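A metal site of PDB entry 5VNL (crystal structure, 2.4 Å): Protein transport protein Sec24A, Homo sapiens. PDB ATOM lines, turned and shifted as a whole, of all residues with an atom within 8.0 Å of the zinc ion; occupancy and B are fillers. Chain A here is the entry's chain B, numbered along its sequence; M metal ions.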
ATOM      1  N   ARG A  85      -6.956  20.590 -16.279  1.00  0.00           N
ATOM      2  CA  ARG A  85      -6.528  21.181 -15.007  1.00  0.00           C
ATOM      3  C   ARG A  85      -6.084  22.606 -15.254  1.00  0.00           C
ATOM      4  O   ARG A  85      -5.511  22.916 -16.301  1.00  0.00           O
ATOM      5  CB  ARG A  85      -5.394  20.366 -14.372  1.00  0.00           C
ATOM      6  CG  ARG A  85      -5.724  18.895 -14.161  1.00  0.00           C
ATOM      7  CD  ARG A  85      -4.544  18.152 -13.547  1.00  0.00           C
ATOM      8  NE  ARG A  85      -4.281  18.590 -12.187  1.00  0.00           N
ATOM      9  CZ  ARG A  85      -3.353  18.050 -11.395  1.00  0.00           C
ATOM     10  NH1 ARG A  85      -2.609  17.041 -11.829  1.00  0.00           N
ATOM     11  NH2 ARG A  85      -3.176  18.531 -10.164  1.00  0.00           N
ATOM     12  N   CYS A  86      -6.360  23.480 -14.289  1.00  0.00           N
ATOM     13  CA  CYS A  86      -5.967  24.888 -14.426  1.00  0.00           C
ATOM     14  C   CYS A  86      -4.451  24.991 -14.581  1.00  0.00           C
ATOM     15  O   CYS A  86      -3.690  24.405 -13.817  1.00  0.00           O
ATOM     16  CB  CYS A  86      -6.429  25.683 -13.210  1.00  0.00           C
ATOM     17  SG  CYS A  86      -5.640  27.295 -13.087  1.00  0.00           S
ATOM     18  N   ARG A  87      -4.028  25.770 -15.581  1.00  0.00           N
ATOM     19  CA  ARG A  87      -2.611  25.865 -15.914  1.00  0.00           C
ATOM     20  C   ARG A  87      -1.768  26.463 -14.799  1.00  0.00           C
ATOM     21  O   ARG A  87      -0.540  26.318 -14.818  1.00  0.00           O
ATOM     22  CB  ARG A  87      -2.425  26.692 -17.193  1.00  0.00           C
ATOM     23  CG  ARG A  87      -2.871  26.000 -18.463  1.00  0.00           C
ATOM     24  CD  ARG A  87      -2.540  26.853 -19.682  1.00  0.00           C
ATOM     25  NE  ARG A  87      -2.960  26.226 -20.929  1.00  0.00           N
ATOM     26  CZ  ARG A  87      -2.822  26.789 -22.123  1.00  0.00           C
ATOM     27  NH1 ARG A  87      -2.274  27.992 -22.243  1.00  0.00           N
ATOM     28  NH2 ARG A  87      -3.235  26.145 -23.219  1.00  0.00           N
ATOM     29  N   SER A  88      -2.383  27.140 -13.818  1.00  0.00           N
ATOM     30  CA  SER A  88      -1.644  27.786 -12.741  1.00  0.00           C
ATOM     31  C   SER A  88      -1.550  26.923 -11.490  1.00  0.00           C
ATOM     32  O   SER A  88      -0.447  26.546 -11.080  1.00  0.00           O
ATOM     33  CB  SER A  88      -2.288  29.140 -12.407  1.00  0.00           C
ATOM     34  OG  SER A  88      -1.820  30.165 -13.267  1.00  0.00           O
ATOM     35  N   CYS A  89      -2.686  26.600 -10.864  1.00  0.00           N
ATOM     36  CA  CYS A  89      -2.707  25.893  -9.592  1.00  0.00           C
ATOM     37  C   CYS A  89      -3.035  24.411  -9.729  1.00  0.00           C
ATOM     38  O   CYS A  89      -3.206  23.735  -8.715  1.00  0.00           O
ATOM     39  CB  CYS A  89      -3.705  26.562  -8.649  1.00  0.00           C
ATOM     40  SG  CYS A  89      -5.417  26.389  -9.193  1.00  0.00           S
ATOM     41  N   ARG A  90      -3.157  23.911 -10.964  1.00  0.00           N
ATOM     42  CA  ARG A  90      -3.408  22.495 -11.250  1.00  0.00           C
ATOM     43  C   ARG A  90      -4.742  22.001 -10.675  1.00  0.00           C
ATOM     44  O   ARG A  90      -4.907  20.798 -10.464  1.00  0.00           O
ATOM     45  CB  ARG A  90      -2.263  21.613 -10.758  1.00  0.00           C
ATOM     46  CG  ARG A  90      -0.872  22.032 -11.228  1.00  0.00           C
ATOM     47  CD  ARG A  90      -0.807  22.261 -12.733  1.00  0.00           C
ATOM     48  NE  ARG A  90      -1.492  21.224 -13.506  1.00  0.00           N
ATOM     49  CZ  ARG A  90      -0.923  20.091 -13.912  1.00  0.00           C
ATOM     50  NH1 ARG A  90       0.350  19.832 -13.603  1.00  0.00           N
ATOM     51  NH2 ARG A  90      -1.615  19.209 -14.608  1.00  0.00           N
ATOM     52  N   THR A  91      -5.691  22.891 -10.422  1.00  0.00           N
ATOM     53  CA  THR A  91      -7.015  22.469  -9.967  1.00  0.00           C
ATOM     54  C   THR A  91      -7.761  21.761 -11.095  1.00  0.00           C
ATOM     55  O   THR A  91      -7.749  22.209 -12.236  1.00  0.00           O
ATOM     56  CB  THR A  91      -7.810  23.675  -9.478  1.00  0.00           C
ATOM     57  OG1 THR A  91      -7.219  24.212  -8.293  1.00  0.00           O
ATOM     58  CG2 THR A  91      -9.258  23.304  -9.188  1.00  0.00           C
ATOM     59  N   TYR A  92      -8.406  20.656 -10.753  1.00  0.00           N
ATOM     60  CA  TYR A  92      -9.188  19.913 -11.744  1.00  0.00           C
ATOM     61  C   TYR A  92     -10.470  20.654 -12.082  1.00  0.00           C
ATOM     62  O   TYR A  92     -11.117  21.237 -11.205  1.00  0.00           O
ATOM     63  CB  TYR A  92      -9.507  18.515 -11.228  1.00  0.00           C
ATOM     64  CG  TYR A  92      -8.291  17.653 -11.042  1.00  0.00           C
ATOM     65  CD1 TYR A  92      -7.550  17.709  -9.864  1.00  0.00           C
ATOM     66  CD2 TYR A  92      -7.890  16.776 -12.030  1.00  0.00           C
ATOM     67  CE1 TYR A  92      -6.432  16.908  -9.697  1.00  0.00           C
ATOM     68  CE2 TYR A  92      -6.777  15.983 -11.872  1.00  0.00           C
ATOM     69  CZ  TYR A  92      -6.055  16.050 -10.707  1.00  0.00           C
ATOM     70  OH  TYR A  92      -4.940  15.254 -10.563  1.00  0.00           O
ATOM     71  N   TRP A 105     -12.531  29.135 -19.498  1.00  0.00           N
ATOM     72  CA  TRP A 105     -13.154  28.946 -18.194  1.00  0.00           C
ATOM     73  C   TRP A 105     -12.275  29.526 -17.092  1.00  0.00           C
ATOM     74  O   TRP A 105     -11.052  29.343 -17.102  1.00  0.00           O
ATOM     75  CB  TRP A 105     -13.416  27.464 -17.906  1.00  0.00           C
ATOM     76  CG  TRP A 105     -12.192  26.579 -17.853  1.00  0.00           C
ATOM     77  CD1 TRP A 105     -11.556  25.994 -18.914  1.00  0.00           C
ATOM     78  CD2 TRP A 105     -11.480  26.161 -16.681  1.00  0.00           C
ATOM     79  NE1 TRP A 105     -10.497  25.247 -18.473  1.00  0.00           N
ATOM     80  CE2 TRP A 105     -10.424  25.329 -17.107  1.00  0.00           C
ATOM     81  CE3 TRP A 105     -11.632  26.420 -15.311  1.00  0.00           C
ATOM     82  CZ2 TRP A 105      -9.520  24.754 -16.213  1.00  0.00           C
ATOM     83  CZ3 TRP A 105     -10.734  25.845 -14.425  1.00  0.00           C
ATOM     84  CH2 TRP A 105      -9.688  25.017 -14.881  1.00  0.00           C
ATOM     85  N   LYS A 106     -12.907  30.210 -16.137  1.00  0.00           N
ATOM     86  CA  LYS A 106     -12.209  30.883 -15.056  1.00  0.00           C
ATOM     87  C   LYS A 106     -12.059  29.935 -13.866  1.00  0.00           C
ATOM     88  O   LYS A 106     -13.065  29.462 -13.313  1.00  0.00           O
ATOM     89  CB  LYS A 106     -12.930  32.155 -14.636  1.00  0.00           C
ATOM     90  CG  LYS A 106     -12.416  32.731 -13.329  1.00  0.00           C
ATOM     91  CD  LYS A 106     -13.060  34.063 -13.004  1.00  0.00           C
ATOM     92  CE  LYS A 106     -12.505  35.168 -13.868  1.00  0.00           C
ATOM     93  NZ  LYS A 106     -13.152  36.467 -13.550  1.00  0.00           N
ATOM     94  N   CYS A 107     -10.819  29.695 -13.455  1.00  0.00           N
ATOM     95  CA  CYS A 107     -10.539  28.782 -12.348  1.00  0.00           C
ATOM     96  C   CYS A 107     -11.119  29.324 -11.043  1.00  0.00           C
ATOM     97  O   CYS A 107     -10.863  30.478 -10.675  1.00  0.00           O
ATOM     98  CB  CYS A 107      -9.031  28.560 -12.223  1.00  0.00           C
ATOM     99  SG  CYS A 107      -8.495  27.501 -10.839  1.00  0.00           S
ATOM    100  N   ASN A 108     -11.901  28.499 -10.355  1.00  0.00           N
ATOM    101  CA  ASN A 108     -12.563  28.959  -9.140  1.00  0.00           C
ATOM    102  C   ASN A 108     -11.638  28.968  -7.924  1.00  0.00           C
ATOM    103  O   ASN A 108     -12.078  29.395  -6.847  1.00  0.00           O
ATOM    104  CB  ASN A 108     -13.780  28.080  -8.843  1.00  0.00           C
ATOM    105  CG  ASN A 108     -13.441  26.607  -8.811  1.00  0.00           C
ATOM    106  OD1 ASN A 108     -12.493  26.162  -9.457  1.00  0.00           O
ATOM    107  ND2 ASN A 108     -14.225  25.838  -8.064  1.00  0.00           N
ATOM    108  N   LEU A 109     -10.389  28.541  -8.067  1.00  0.00           N
ATOM    109  CA  LEU A 109      -9.459  28.558  -6.947  1.00  0.00           C
ATOM    110  C   LEU A 109      -8.347  29.596  -7.077  1.00  0.00           C
ATOM    111  O   LEU A 109      -7.894  30.111  -6.061  1.00  0.00           O
ATOM    112  CB  LEU A 109      -8.841  27.175  -6.727  1.00  0.00           C
ATOM    113  CG  LEU A 109      -9.664  26.245  -5.810  1.00  0.00           C
ATOM    114  CD1 LEU A 109     -10.940  25.774  -6.475  1.00  0.00           C
ATOM    115  CD2 LEU A 109      -8.837  25.059  -5.383  1.00  0.00           C
ATOM    116  N   CYS A 110      -7.914  29.925  -8.298  1.00  0.00           N
ATOM    117  CA  CYS A 110      -6.906  30.973  -8.447  1.00  0.00           C
ATOM    118  C   CYS A 110      -7.294  32.006  -9.508  1.00  0.00           C
ATOM    119  O   CYS A 110      -6.445  32.824  -9.887  1.00  0.00           O
ATOM    120  CB  CYS A 110      -5.544  30.358  -8.787  1.00  0.00           C
ATOM    121  SG  CYS A 110      -5.372  29.758 -10.478  1.00  0.00           S
ATOM    122  N   TYR A 111      -8.527  31.995 -10.008  1.00  0.00           N
ATOM    123  CA  TYR A 111      -9.151  33.005 -10.874  1.00  0.00           C
ATOM    124  C   TYR A 111      -8.510  33.142 -12.252  1.00  0.00           C
ATOM    125  O   TYR A 111      -8.939  34.011 -13.026  1.00  0.00           O
ATOM    126  CB  TYR A 111      -9.193  34.381 -10.190  1.00  0.00           C
ATOM    127  CG  TYR A 111      -9.737  34.323  -8.771  1.00  0.00           C
ATOM    128  CD1 TYR A 111     -10.856  33.567  -8.466  1.00  0.00           C
ATOM    129  CD2 TYR A 111      -9.109  35.014  -7.739  1.00  0.00           C
ATOM    130  CE1 TYR A 111     -11.347  33.500  -7.179  1.00  0.00           C
ATOM    131  CE2 TYR A 111      -9.601  34.961  -6.441  1.00  0.00           C
ATOM    132  CZ  TYR A 111     -10.723  34.197  -6.171  1.00  0.00           C
ATOM    133  OH  TYR A 111     -11.243  34.121  -4.899  1.00  0.00           O
ATOM    134  N   ARG A 112      -7.523  32.321 -12.584  1.00  0.00           N
ATOM    135  CA  ARG A 112      -6.917  32.393 -13.912  1.00  0.00           C
ATOM    136  C   ARG A 112      -7.851  31.821 -14.970  1.00  0.00           C
ATOM    137  O   ARG A 112      -8.555  30.833 -14.738  1.00  0.00           O
ATOM    138  CB  ARG A 112      -5.582  31.639 -13.940  1.00  0.00           C
ATOM    139  CG  ARG A 112      -5.273  30.962 -15.267  1.00  0.00           C
ATOM    140  CD  ARG A 112      -3.781  30.930 -15.567  1.00  0.00           C
ATOM    141  NE  ARG A 112      -3.533  30.649 -16.973  1.00  0.00           N
ATOM    142  CZ  ARG A 112      -2.341  30.415 -17.508  1.00  0.00           C
ATOM    143  NH1 ARG A 112      -1.250  30.428 -16.738  1.00  0.00           N
ATOM    144  NH2 ARG A 112      -2.232  30.168 -18.806  1.00  0.00           N
ATOM    145  N   VAL A 113      -7.858  32.451 -16.145  1.00  0.00           N
ATOM    146  CA  VAL A 113      -8.664  31.990 -17.269  1.00  0.00           C
ATOM    147  C   VAL A 113      -7.891  30.919 -18.030  1.00  0.00           C
ATOM    148  O   VAL A 113      -6.698  31.070 -18.304  1.00  0.00           O
ATOM    149  CB  VAL A 113      -9.041  33.173 -18.177  1.00  0.00           C
ATOM    150  CG1 VAL A 113     -10.087  32.752 -19.190  1.00  0.00           C
ATOM    151  CG2 VAL A 113      -9.523  34.328 -17.328  1.00  0.00           C
ATOM    152  N   ASN A 114      -8.575  29.821 -18.369  1.00  0.00           N
ATOM    153  CA  ASN A 114      -7.971  28.704 -19.076  1.00  0.00           C
ATOM    154  C   ASN A 114      -8.719  28.432 -20.375  1.00  0.00           C
ATOM    155  O   ASN A 114      -9.923  28.709 -20.483  1.00  0.00           O
ATOM    156  CB  ASN A 114      -7.970  27.425 -18.227  1.00  0.00           C
ATOM    157  CG  ASN A 114      -6.858  27.414 -17.199  1.00  0.00           C
ATOM    158  OD1 ASN A 114      -5.771  26.891 -17.444  1.00  0.00           O
ATOM    159  ND2 ASN A 114      -7.127  28.003 -16.035  1.00  0.00           N
ATOM    160  N   ARG A 407      -6.774  21.442  -1.893  1.00  0.00           N
ATOM    161  CA  ARG A 407      -6.704  22.792  -2.409  1.00  0.00           C
ATOM    162  C   ARG A 407      -7.913  23.596  -1.933  1.00  0.00           C
ATOM    163  O   ARG A 407      -8.989  23.048  -1.728  1.00  0.00           O
ATOM    164  CB  ARG A 407      -6.637  22.807  -3.939  1.00  0.00           C
ATOM    165  CG  ARG A 407      -5.350  22.304  -4.542  1.00  0.00           C
ATOM    166  CD  ARG A 407      -5.387  22.428  -6.067  1.00  0.00           C
ATOM    167  NE  ARG A 407      -4.185  21.899  -6.702  1.00  0.00           N
ATOM    168  CZ  ARG A 407      -4.013  20.609  -6.999  1.00  0.00           C
ATOM    169  NH1 ARG A 407      -4.962  19.728  -6.724  1.00  0.00           N
ATOM    170  NH2 ARG A 407      -2.883  20.206  -7.578  1.00  0.00           N
HETATM  171 ZN    ZN M   1      -6.209  27.784 -10.968  1.00  0.00          ZN
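The backbone NH of Cys 86 is in hydrogen-bond range of the backbone carbonyl oxygen of Thr 91 (2.8 Å).
The backbone NH (N) of Ser 88 lies close to the side-chain sulfur (SG) of Cys 86, at 3.3 Å.
The side-chain sulfur (SG) of Cys 86 sits close to the side-chain amide nitrogen (ND2) of Asn 114 (3.4 Å).
The backbone NH (N) of Leu 109 sits close to the side-chain sulfur (SG) of Cys 107 (3.5 Å).
The side-chain sulfur (SG) of Cys 89 lies close to the side-chain hydroxyl (OG1) of Thr 91 (3.0 Å).
O of Cys 89 is in hydrogen-bond range of NE of Arg 407, at 2.9 Å.
N of Cys 107 lies within hydrogen-bond range of O of Arg 112 (2.8 Å).
The nearest printed residue that does not touch the zinc ion is Ser 88 (4.4 Å).
The zinc ion is bound by SG of Cys 110.
SG of Cys 86 binds the zinc ion (2.2 Å).
The zinc ion is bound by SG of Cys 107 (2.3 Å).
SG of Cys 89 is bound to the zinc ion.
The zinc ion has four donor atoms within binding distance.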
